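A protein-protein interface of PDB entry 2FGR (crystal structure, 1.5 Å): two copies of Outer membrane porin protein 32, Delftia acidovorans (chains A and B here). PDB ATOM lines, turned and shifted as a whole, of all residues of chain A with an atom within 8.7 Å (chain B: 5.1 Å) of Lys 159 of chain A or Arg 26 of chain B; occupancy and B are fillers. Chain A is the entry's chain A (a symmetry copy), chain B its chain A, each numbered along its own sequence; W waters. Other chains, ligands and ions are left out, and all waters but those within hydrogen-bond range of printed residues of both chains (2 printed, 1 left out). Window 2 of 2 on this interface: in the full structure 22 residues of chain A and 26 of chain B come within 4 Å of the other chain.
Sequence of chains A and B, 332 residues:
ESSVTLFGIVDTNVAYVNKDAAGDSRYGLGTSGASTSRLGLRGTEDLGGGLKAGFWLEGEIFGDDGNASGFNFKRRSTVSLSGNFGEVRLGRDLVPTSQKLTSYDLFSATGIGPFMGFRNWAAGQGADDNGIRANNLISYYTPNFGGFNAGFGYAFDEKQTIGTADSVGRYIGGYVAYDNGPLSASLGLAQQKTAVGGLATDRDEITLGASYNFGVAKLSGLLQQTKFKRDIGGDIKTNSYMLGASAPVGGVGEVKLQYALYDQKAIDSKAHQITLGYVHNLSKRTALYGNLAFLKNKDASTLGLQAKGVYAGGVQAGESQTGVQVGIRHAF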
ATOM      1  N   ASN A 136       4.020   5.713  -8.603  1.00  0.00           N
ATOM      2  CA  ASN A 136       2.586   5.769  -8.768  1.00  0.00           C
ATOM      3  C   ASN A 136       1.831   5.799  -7.439  1.00  0.00           C
ATOM      4  O   ASN A 136       0.717   5.278  -7.338  1.00  0.00           O
ATOM      5  CB  ASN A 136       2.061   4.615  -9.638  1.00  0.00           C
ATOM      6  CG  ASN A 136       2.874   4.467 -10.929  1.00  0.00           C
ATOM      7  OD1 ASN A 136       3.118   5.473 -11.605  1.00  0.00           O
ATOM      8  ND2 ASN A 136       3.309   3.242 -11.252  1.00  0.00           N
ATOM      9  N   PHE A 156      -0.456   2.398  -7.583  1.00  0.00           N
ATOM     10  CA  PHE A 156      -1.037   1.743  -8.744  1.00  0.00           C
ATOM     11  C   PHE A 156      -0.018   0.872  -9.462  1.00  0.00           C
ATOM     12  O   PHE A 156       1.085   1.318  -9.759  1.00  0.00           O
ATOM     13  CB  PHE A 156      -1.582   2.768  -9.747  1.00  0.00           C
ATOM     14  CG  PHE A 156      -2.667   3.632  -9.219  1.00  0.00           C
ATOM     15  CD1 PHE A 156      -2.383   4.851  -8.667  1.00  0.00           C
ATOM     16  CD2 PHE A 156      -4.007   3.229  -9.280  1.00  0.00           C
ATOM     17  CE1 PHE A 156      -3.405   5.680  -8.190  1.00  0.00           C
ATOM     18  CE2 PHE A 156      -5.007   4.039  -8.798  1.00  0.00           C
ATOM     19  CZ  PHE A 156      -4.706   5.275  -8.252  1.00  0.00           C
ATOM     20  N   ASP A 157      -0.422  -0.352  -9.808  1.00  0.00           N
ATOM     21  CA  ASP A 157       0.403  -1.241 -10.619  1.00  0.00           C
ATOM     22  C   ASP A 157       0.409  -0.914 -12.085  1.00  0.00           C
ATOM     23  O   ASP A 157       1.383  -1.208 -12.785  1.00  0.00           O
ATOM     24  CB  ASP A 157      -0.073  -2.695 -10.464  1.00  0.00           C
ATOM     25  CG  ASP A 157      -1.554  -2.824 -10.669  1.00  0.00           C
ATOM     26  OD1 ASP A 157      -1.990  -3.152 -11.810  1.00  0.00           O
ATOM     27  OD2 ASP A 157      -2.382  -2.523  -9.758  1.00  0.00           O
ATOM     28  N   GLU A 158      -0.688  -0.328 -12.549  1.00  0.00           N
ATOM     29  CA  GLU A 158      -0.837   0.075 -13.959  1.00  0.00           C
ATOM     30  C   GLU A 158      -0.642  -1.106 -14.920  1.00  0.00           C
ATOM     31  O   GLU A 158      -0.138  -0.950 -16.039  1.00  0.00           O
ATOM     32  CB  GLU A 158       0.101   1.236 -14.304  1.00  0.00           C
ATOM     33  CG  GLU A 158      -0.081   2.390 -13.350  1.00  0.00           C
ATOM     34  CD  GLU A 158       0.807   3.607 -13.548  1.00  0.00           C
ATOM     35  OE1 GLU A 158       1.858   3.565 -14.255  1.00  0.00           O
ATOM     36  OE2 GLU A 158       0.454   4.632 -12.929  1.00  0.00           O
ATOM     37  N   LYS A 159      -1.064  -2.276 -14.461  1.00  0.00           N
ATOM     38  CA  LYS A 159      -1.021  -3.526 -15.247  1.00  0.00           C
ATOM     39  C   LYS A 159       0.420  -3.950 -15.636  1.00  0.00           C
ATOM     40  O   LYS A 159       0.632  -4.657 -16.606  1.00  0.00           O
ATOM     41  CB  LYS A 159      -1.974  -3.426 -16.475  1.00  0.00           C
ATOM     42  CG  LYS A 159      -2.489  -4.728 -17.131  1.00  0.00           C
ATOM     43  CD  LYS A 159      -3.351  -4.468 -18.487  1.00  0.00           C
ATOM     44  CE  LYS A 159      -2.800  -5.141 -19.805  1.00  0.00           C
ATOM     45  NZ  LYS A 159      -3.655  -5.064 -21.231  1.00  0.00           N
ATOM     46  N   GLN A 160       1.425  -3.535 -14.868  1.00  0.00           N
ATOM     47  CA  GLN A 160       2.765  -4.037 -15.069  1.00  0.00           C
ATOM     48  C   GLN A 160       2.733  -5.552 -14.938  1.00  0.00           C
ATOM     49  O   GLN A 160       2.229  -6.095 -13.959  1.00  0.00           O
ATOM     50  CB  GLN A 160       3.792  -3.437 -14.112  1.00  0.00           C
ATOM     51  CG  GLN A 160       5.182  -3.925 -14.425  1.00  0.00           C
ATOM     52  CD  GLN A 160       6.261  -3.615 -13.412  1.00  0.00           C
ATOM     53  OE1 GLN A 160       7.408  -4.034 -13.620  1.00  0.00           O
ATOM     54  NE2 GLN A 160       5.925  -2.915 -12.320  1.00  0.00           N
ATOM     55  N   THR A 161       3.221  -6.217 -15.977  1.00  0.00           N
ATOM     56  CA  THR A 161       3.142  -7.647 -16.079  1.00  0.00           C
ATOM     57  C   THR A 161       4.473  -8.327 -16.218  1.00  0.00           C
ATOM     58  O   THR A 161       5.303  -7.957 -17.080  1.00  0.00           O
ATOM     59  CB  THR A 161       2.242  -8.004 -17.238  1.00  0.00           C
ATOM     60  OG1 THR A 161       2.720  -7.415 -18.443  1.00  0.00           O
ATOM     61  CG2 THR A 161       0.912  -7.440 -17.076  1.00  0.00           C
ATOM     62  N   ILE A 162       4.703  -9.290 -15.320  1.00  0.00           N
ATOM     63  CA  ILE A 162       5.895 -10.129 -15.344  1.00  0.00           C
ATOM     64  C   ILE A 162       5.396 -11.544 -15.139  1.00  0.00           C
ATOM     65  O   ILE A 162       4.884 -11.867 -14.071  1.00  0.00           O
ATOM     66  CB  ILE A 162       6.908  -9.786 -14.251  1.00  0.00           C
ATOM     67  CG1 ILE A 162       7.331  -8.303 -14.333  1.00  0.00           C
ATOM     68  CG2 ILE A 162       8.124 -10.747 -14.331  1.00  0.00           C
ATOM     69  CD1 ILE A 162       8.289  -7.889 -13.291  1.00  0.00           C
ATOM     70  N   ALA A 165       2.124 -12.559 -13.100  1.00  0.00           N
ATOM     71  CA  ALA A 165       1.708 -11.411 -12.312  1.00  0.00           C
ATOM     72  C   ALA A 165       1.351 -10.262 -13.234  1.00  0.00           C
ATOM     73  O   ALA A 165       2.203  -9.788 -13.999  1.00  0.00           O
ATOM     74  CB  ALA A 165       2.823 -10.978 -11.378  1.00  0.00           C
ATOM     75  N   ASP A 166       0.105  -9.818 -13.151  1.00  0.00           N
ATOM     76  CA  ASP A 166      -0.334  -8.681 -13.952  1.00  0.00           C
ATOM     77  C   ASP A 166      -0.643  -7.431 -13.158  1.00  0.00           C
ATOM     78  O   ASP A 166      -1.282  -6.494 -13.702  1.00  0.00           O
ATOM     79  CB  ASP A 166      -1.487  -9.045 -14.901  1.00  0.00           C
ATOM     80  CG  ASP A 166      -2.745  -9.374 -14.188  1.00  0.00           C
ATOM     81  OD1 ASP A 166      -2.726  -9.442 -12.937  1.00  0.00           O
ATOM     82  OD2 ASP A 166      -3.826  -9.552 -14.824  1.00  0.00           O
ATOM     83  N   SER A 167      -0.159  -7.376 -11.905  1.00  0.00           N
ATOM     84  CA  SER A 167      -0.309  -6.187 -11.085  1.00  0.00           C
ATOM     85  C   SER A 167       0.979  -5.870 -10.324  1.00  0.00           C
ATOM     86  O   SER A 167       0.963  -5.395  -9.159  1.00  0.00           O
ATOM     87  CB  SER A 167      -1.486  -6.332 -10.147  1.00  0.00           C
ATOM     88  OG  SER A 167      -1.355  -7.453  -9.276  1.00  0.00           O
ATOM     89  N   VAL A 168       2.119  -6.096 -10.980  1.00  0.00           N
ATOM     90  CA  VAL A 168       3.409  -5.903 -10.338  1.00  0.00           C
ATOM     91  C   VAL A 168       3.566  -4.450  -9.921  1.00  0.00           C
ATOM     92  O   VAL A 168       3.228  -3.554 -10.665  1.00  0.00           O
ATOM     93  CB  VAL A 168       4.582  -6.299 -11.240  1.00  0.00           C
ATOM     94  CG1 VAL A 168       5.936  -6.040 -10.562  1.00  0.00           C
ATOM     95  CG2 VAL A 168       4.470  -7.795 -11.598  1.00  0.00           C
ATOM     96  N   GLY A 169       4.020  -4.237  -8.693  1.00  0.00           N
ATOM     97  CA  GLY A 169       4.253  -2.887  -8.214  1.00  0.00           C
ATOM     98  C   GLY A 169       3.121  -2.299  -7.373  1.00  0.00           C
ATOM     99  O   GLY A 169       3.291  -1.249  -6.722  1.00  0.00           O
ATOM    100  N   ARG A 170       1.966  -2.951  -7.347  1.00  0.00           N
ATOM    101  CA  ARG A 170       0.901  -2.480  -6.464  1.00  0.00           C
ATOM    102  C   ARG A 170       1.399  -2.433  -5.025  1.00  0.00           C
ATOM    103  O   ARG A 170       2.048  -3.374  -4.569  1.00  0.00           O
ATOM    104  CB  ARG A 170      -0.338  -3.350  -6.588  1.00  0.00           C
ATOM    105  CG  ARG A 170      -1.553  -2.801  -5.869  1.00  0.00           C
ATOM    106  CD  ARG A 170      -2.742  -3.706  -5.910  1.00  0.00           C
ATOM    107  NE  ARG A 170      -3.194  -3.871  -7.284  1.00  0.00           N
ATOM    108  CZ  ARG A 170      -4.086  -4.768  -7.675  1.00  0.00           C
ATOM    109  NH1 ARG A 170      -4.580  -5.660  -6.805  1.00  0.00           N
ATOM    110  NH2 ARG A 170      -4.449  -4.799  -8.949  1.00  0.00           N
ATOM    111  N   ALA B  15      -5.453   8.879 -13.617  1.00  0.00           N
ATOM    112  CA  ALA B  15      -6.002   8.773 -14.956  1.00  0.00           C
ATOM    113  C   ALA B  15      -6.516   7.360 -15.253  1.00  0.00           C
ATOM    114  O   ALA B  15      -6.118   6.397 -14.638  1.00  0.00           O
ATOM    115  CB  ALA B  15      -4.968   9.148 -15.997  1.00  0.00           C
ATOM    116  N   TYR B  16      -7.431   7.295 -16.196  1.00  0.00           N
ATOM    117  CA  TYR B  16      -8.098   6.075 -16.599  1.00  0.00           C
ATOM    118  C   TYR B  16      -8.348   6.142 -18.105  1.00  0.00           C
ATOM    119  O   TYR B  16      -8.772   7.188 -18.626  1.00  0.00           O
ATOM    120  CB  TYR B  16      -9.418   5.973 -15.829  1.00  0.00           C
ATOM    121  CG  TYR B  16     -10.398   4.970 -16.356  1.00  0.00           C
ATOM    122  CD1 TYR B  16     -11.353   5.342 -17.301  1.00  0.00           C
ATOM    123  CD2 TYR B  16     -10.395   3.678 -15.920  1.00  0.00           C
ATOM    124  CE1 TYR B  16     -12.262   4.428 -17.795  1.00  0.00           C
ATOM    125  CE2 TYR B  16     -11.295   2.747 -16.419  1.00  0.00           C
ATOM    126  CZ  TYR B  16     -12.224   3.137 -17.350  1.00  0.00           C
ATOM    127  OH  TYR B  16     -13.139   2.221 -17.826  1.00  0.00           O
ATOM    128  N   VAL B  17      -8.142   5.023 -18.789  1.00  0.00           N
ATOM    129  CA  VAL B  17      -8.679   4.834 -20.136  1.00  0.00           C
ATOM    130  C   VAL B  17      -9.438   3.522 -20.140  1.00  0.00           C
ATOM    131  O   VAL B  17      -9.056   2.567 -19.473  1.00  0.00           O
ATOM    132  CB  VAL B  17      -7.616   4.843 -21.233  1.00  0.00           C
ATOM    133  CG1 VAL B  17      -6.964   6.185 -21.298  1.00  0.00           C
ATOM    134  CG2 VAL B  17      -6.589   3.753 -21.056  1.00  0.00           C
ATOM    135  N   ASN B  18     -10.521   3.455 -20.897  1.00  0.00           N
ATOM    136  CA  ASN B  18     -11.352   2.236 -20.848  1.00  0.00           C
ATOM    137  C   ASN B  18     -10.817   1.099 -21.688  1.00  0.00           C
ATOM    138  O   ASN B  18     -11.234  -0.049 -21.502  1.00  0.00           O
ATOM    139  CB  ASN B  18     -12.829   2.539 -21.121  1.00  0.00           C
ATOM    140  CG  ASN B  18     -13.144   2.958 -22.552  1.00  0.00           C
ATOM    141  OD1 ASN B  18     -14.378   2.938 -22.986  1.00  0.00           O
ATOM    142  ND2 ASN B  18     -12.160   3.364 -23.283  1.00  0.00           N
ATOM    143  N   ASP B  20      -7.037  -0.367 -23.890  1.00  0.00           N
ATOM    144  CA  ASP B  20      -5.694  -0.332 -24.429  1.00  0.00           C
ATOM    145  C   ASP B  20      -5.658  -1.150 -25.727  1.00  0.00           C
ATOM    146  O   ASP B  20      -6.721  -1.413 -26.329  1.00  0.00           O
ATOM    147  CB  ASP B  20      -4.701  -0.786 -23.362  1.00  0.00           C
ATOM    148  CG  ASP B  20      -4.860  -2.249 -22.949  1.00  0.00           C
ATOM    149  OD1 ASP B  20      -5.625  -3.032 -23.574  1.00  0.00           O
ATOM    150  OD2 ASP B  20      -4.202  -2.691 -21.990  1.00  0.00           O
ATOM    151  N   ALA B  22      -5.129  -4.141 -26.237  1.00  0.00           N
ATOM    152  CA  ALA B  22      -5.772  -5.454 -26.029  1.00  0.00           C
ATOM    153  C   ALA B  22      -7.225  -5.337 -25.597  1.00  0.00           C
ATOM    154  O   ALA B  22      -7.909  -6.346 -25.396  1.00  0.00           O
ATOM    155  CB  ALA B  22      -4.997  -6.258 -25.011  1.00  0.00           C
ATOM    156  N   ASP B  24      -8.329  -3.836 -22.799  1.00  0.00           N
ATOM    157  CA  ASP B  24      -8.463  -3.796 -21.345  1.00  0.00           C
ATOM    158  C   ASP B  24      -8.317  -2.360 -20.822  1.00  0.00           C
ATOM    159  O   ASP B  24      -7.555  -1.588 -21.374  1.00  0.00           O
ATOM    160  CB  ASP B  24      -7.393  -4.649 -20.689  1.00  0.00           C
ATOM    161  CG  ASP B  24      -7.436  -6.084 -21.146  1.00  0.00           C
ATOM    162  OD1 ASP B  24      -8.551  -6.642 -21.280  1.00  0.00           O
ATOM    163  OD2 ASP B  24      -6.403  -6.700 -21.421  1.00  0.00           O
ATOM    164  N   SER B  25      -9.069  -2.028 -19.777  1.00  0.00           N
ATOM    165  CA  SER B  25      -8.938  -0.739 -19.117  1.00  0.00           C
ATOM    166  C   SER B  25      -7.610  -0.612 -18.386  1.00  0.00           C
ATOM    167  O   SER B  25      -6.937  -1.598 -18.050  1.00  0.00           O
ATOM    168  CB  SER B  25     -10.084  -0.486 -18.163  1.00  0.00           C
ATOM    169  OG  SER B  25     -10.092  -1.455 -17.127  1.00  0.00           O
ATOM    170  N   ARG B  26      -7.204   0.632 -18.194  1.00  0.00           N
ATOM    171  CA  ARG B  26      -5.989   0.931 -17.459  1.00  0.00           C
ATOM    172  C   ARG B  26      -6.202   2.159 -16.635  1.00  0.00           C
ATOM    173  O   ARG B  26      -6.839   3.108 -17.041  1.00  0.00           O
ATOM    174  CB  ARG B  26      -4.852   1.184 -18.428  1.00  0.00           C
ATOM    175  CG  ARG B  26      -3.489   1.197 -17.799  1.00  0.00           C
ATOM    176  CD  ARG B  26      -2.707  -0.097 -17.849  1.00  0.00           C
ATOM    177  NE  ARG B  26      -2.656  -0.741 -19.150  1.00  0.00           N
ATOM    178  CZ  ARG B  26      -1.566  -0.866 -19.917  1.00  0.00           C
ATOM    179  NH1 ARG B  26      -0.385  -0.394 -19.543  1.00  0.00           N
ATOM    180  NH2 ARG B  26      -1.645  -1.503 -21.059  1.00  0.00           N
ATOM    181  N   TYR B  27      -5.644   2.146 -15.453  1.00  0.00           N
ATOM    182  CA  TYR B  27      -5.728   3.305 -14.611  1.00  0.00           C
ATOM    183  C   TYR B  27      -4.479   3.404 -13.764  1.00  0.00           C
ATOM    184  O   TYR B  27      -3.752   2.425 -13.582  1.00  0.00           O
ATOM    185  CB  TYR B  27      -6.992   3.296 -13.796  1.00  0.00           C
ATOM    186  CG  TYR B  27      -7.059   2.144 -12.849  1.00  0.00           C
ATOM    187  CD1 TYR B  27      -6.602   2.279 -11.555  1.00  0.00           C
ATOM    188  CD2 TYR B  27      -7.567   0.913 -13.260  1.00  0.00           C
ATOM    189  CE1 TYR B  27      -6.646   1.233 -10.658  1.00  0.00           C
ATOM    190  CE2 TYR B  27      -7.595  -0.188 -12.350  1.00  0.00           C
ATOM    191  CZ  TYR B  27      -7.126  -0.004 -11.056  1.00  0.00           C
ATOM    192  OH  TYR B  27      -7.149  -1.036 -10.120  1.00  0.00           O
ATOM    193  N   GLY B  28      -4.201   4.604 -13.296  1.00  0.00           N
ATOM    194  CA  GLY B  28      -2.988   4.779 -12.559  1.00  0.00           C
ATOM    195  C   GLY B  28      -2.705   6.225 -12.233  1.00  0.00           C
ATOM    196  O   GLY B  28      -3.584   7.052 -12.268  1.00  0.00           O
ATOM    197  N   VAL B 310       0.222   6.635 -17.672  1.00  0.00           N
ATOM    198  CA  VAL B 310      -0.752   5.565 -17.420  1.00  0.00           C
ATOM    199  C   VAL B 310      -0.859   4.709 -18.667  1.00  0.00           C
ATOM    200  O   VAL B 310      -0.500   3.547 -18.633  1.00  0.00           O
ATOM    201  CB  VAL B 310      -2.093   6.119 -16.975  1.00  0.00           C
ATOM    202  CG1 VAL B 310      -3.110   4.958 -16.816  1.00  0.00           C
ATOM    203  CG2 VAL B 310      -1.933   6.790 -15.603  1.00  0.00           C
ATOM    204  N   TYR B 311      -1.334   5.314 -19.760  1.00  0.00           N
ATOM    205  CA  TYR B 311      -1.383   4.620 -21.060  1.00  0.00           C
ATOM    206  C   TYR B 311      -1.497   5.633 -22.178  1.00  0.00           C
ATOM    207  O   TYR B 311      -2.373   6.484 -22.160  1.00  0.00           O
ATOM    208  CB  TYR B 311      -2.554   3.607 -21.115  1.00  0.00           C
ATOM    209  CG  TYR B 311      -2.535   2.799 -22.415  1.00  0.00           C
ATOM    210  CD1 TYR B 311      -1.568   1.832 -22.643  1.00  0.00           C
ATOM    211  CD2 TYR B 311      -3.402   3.094 -23.455  1.00  0.00           C
ATOM    212  CE1 TYR B 311      -1.504   1.135 -23.831  1.00  0.00           C
ATOM    213  CE2 TYR B 311      -3.333   2.395 -24.667  1.00  0.00           C
ATOM    214  CZ  TYR B 311      -2.389   1.423 -24.843  1.00  0.00           C
ATOM    215  OH  TYR B 311      -2.282   0.727 -26.038  1.00  0.00           O
HETATM  216  O   HOH W   1      -3.325   0.356 -11.767  1.00  0.00           O
HETATM  217  O   HOH W   2      -4.185  -0.669  -9.187  1.00  0.00           O
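OD2 of Asp 24 of chain B is in salt-bridge range of NZ of Lys 159 of chain A. The side-chain carboxylate of Asp 20 of chain B lies within salt-bridge range of the side-chain amino group of Lys 159 of chain A (2.6 Å).
Water W2 lies within hydrogen-bond range of the side-chain carboxylate (OD2) of Asp 157 of chain A (2.6 Å) and the side-chain hydroxyl (OH) of Tyr 27 of chain B (3.1 Å). Water W1 lies within hydrogen-bond range of O of Tyr 27 of chain B (2.8 Å) and N of Glu 158 of chain A (2.8 Å).
CD2 of Phe 156 of chain A touches CD1 of Tyr 27 of chain B, 3.6 Å away. Gly 28 of chain B touches Phe 156 of chain A. Glu 158 of chain A touches Arg 26 of chain B (O to CD, 3.3 Å). CG of Glu 158 of chain A touches O of Tyr 27 of chain B, 3.7 Å away. Glu 158 of chain A touches Gly 28 of chain B. Lys 159 of chain A touches Arg 26 of chain B.
Of the 14 printed residues of chain A, 3 touch a printed residue of chain B. Hydrophobic or aromatic side chains of chain A that line the printed part of chain B: Phe 156. Hydrophobic or aromatic side chains of chain B within 4 Å of the printed part of chain A: Tyr 27. Among the printed residues, Asp or Glu carboxylates within 4 Å of a Lys or Arg side-chain nitrogen of the other chain: Lys 159 of chain A with Asp 20 of chain B (2.6 Å) and Lys 159 of chain A with Asp 24 of chain B (3.2 Å).
Of chain A, only Glu 158 and Lys 159 come within 4 Å of Arg 26 of chain B. Ser 25 of chain B touches none of the printed residues of chain A. Of the printed residues of chain A, Asp 24 of chain B touches Lys 159 (3.2 Å). Printed residues of chain A within 4 Å of Asp 20 of chain B: Lys 159 (2.6 Å). Val 17 of chain B touches none of the printed residues of chain A. The nearest residue of chain B that does not touch Lys 159 of chain A is Ala 22 of chain B (4.2 Å). The nearest residue of chain A that does not touch Arg 26 of chain B is Gln 160 of chain A (5.9 Å).
OD1 of Asp 20 of chain B is in hydrogen-bond range of N of Ala 22 of chain B (2.9 Å). OD1 of Asp 157 of chain A lies within hydrogen-bond range of N of Lys 159 of chain A. N of Asp 24 of chain B is in hydrogen-bond range of OD1 of Asp 20 of chain B (2.9 Å). N of Ala 15 of chain B lies within hydrogen-bond range of O of Gly 28 of chain B, 2.9 Å away. O of Asn 136 of chain A sits at hydrogen-bond distance from N of Phe 156 of chain A (3.1 Å). N of Val 17 of chain B lies within hydrogen-bond range of O of Arg 26 of chain B (2.9 Å).
No position is printed for both chains.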
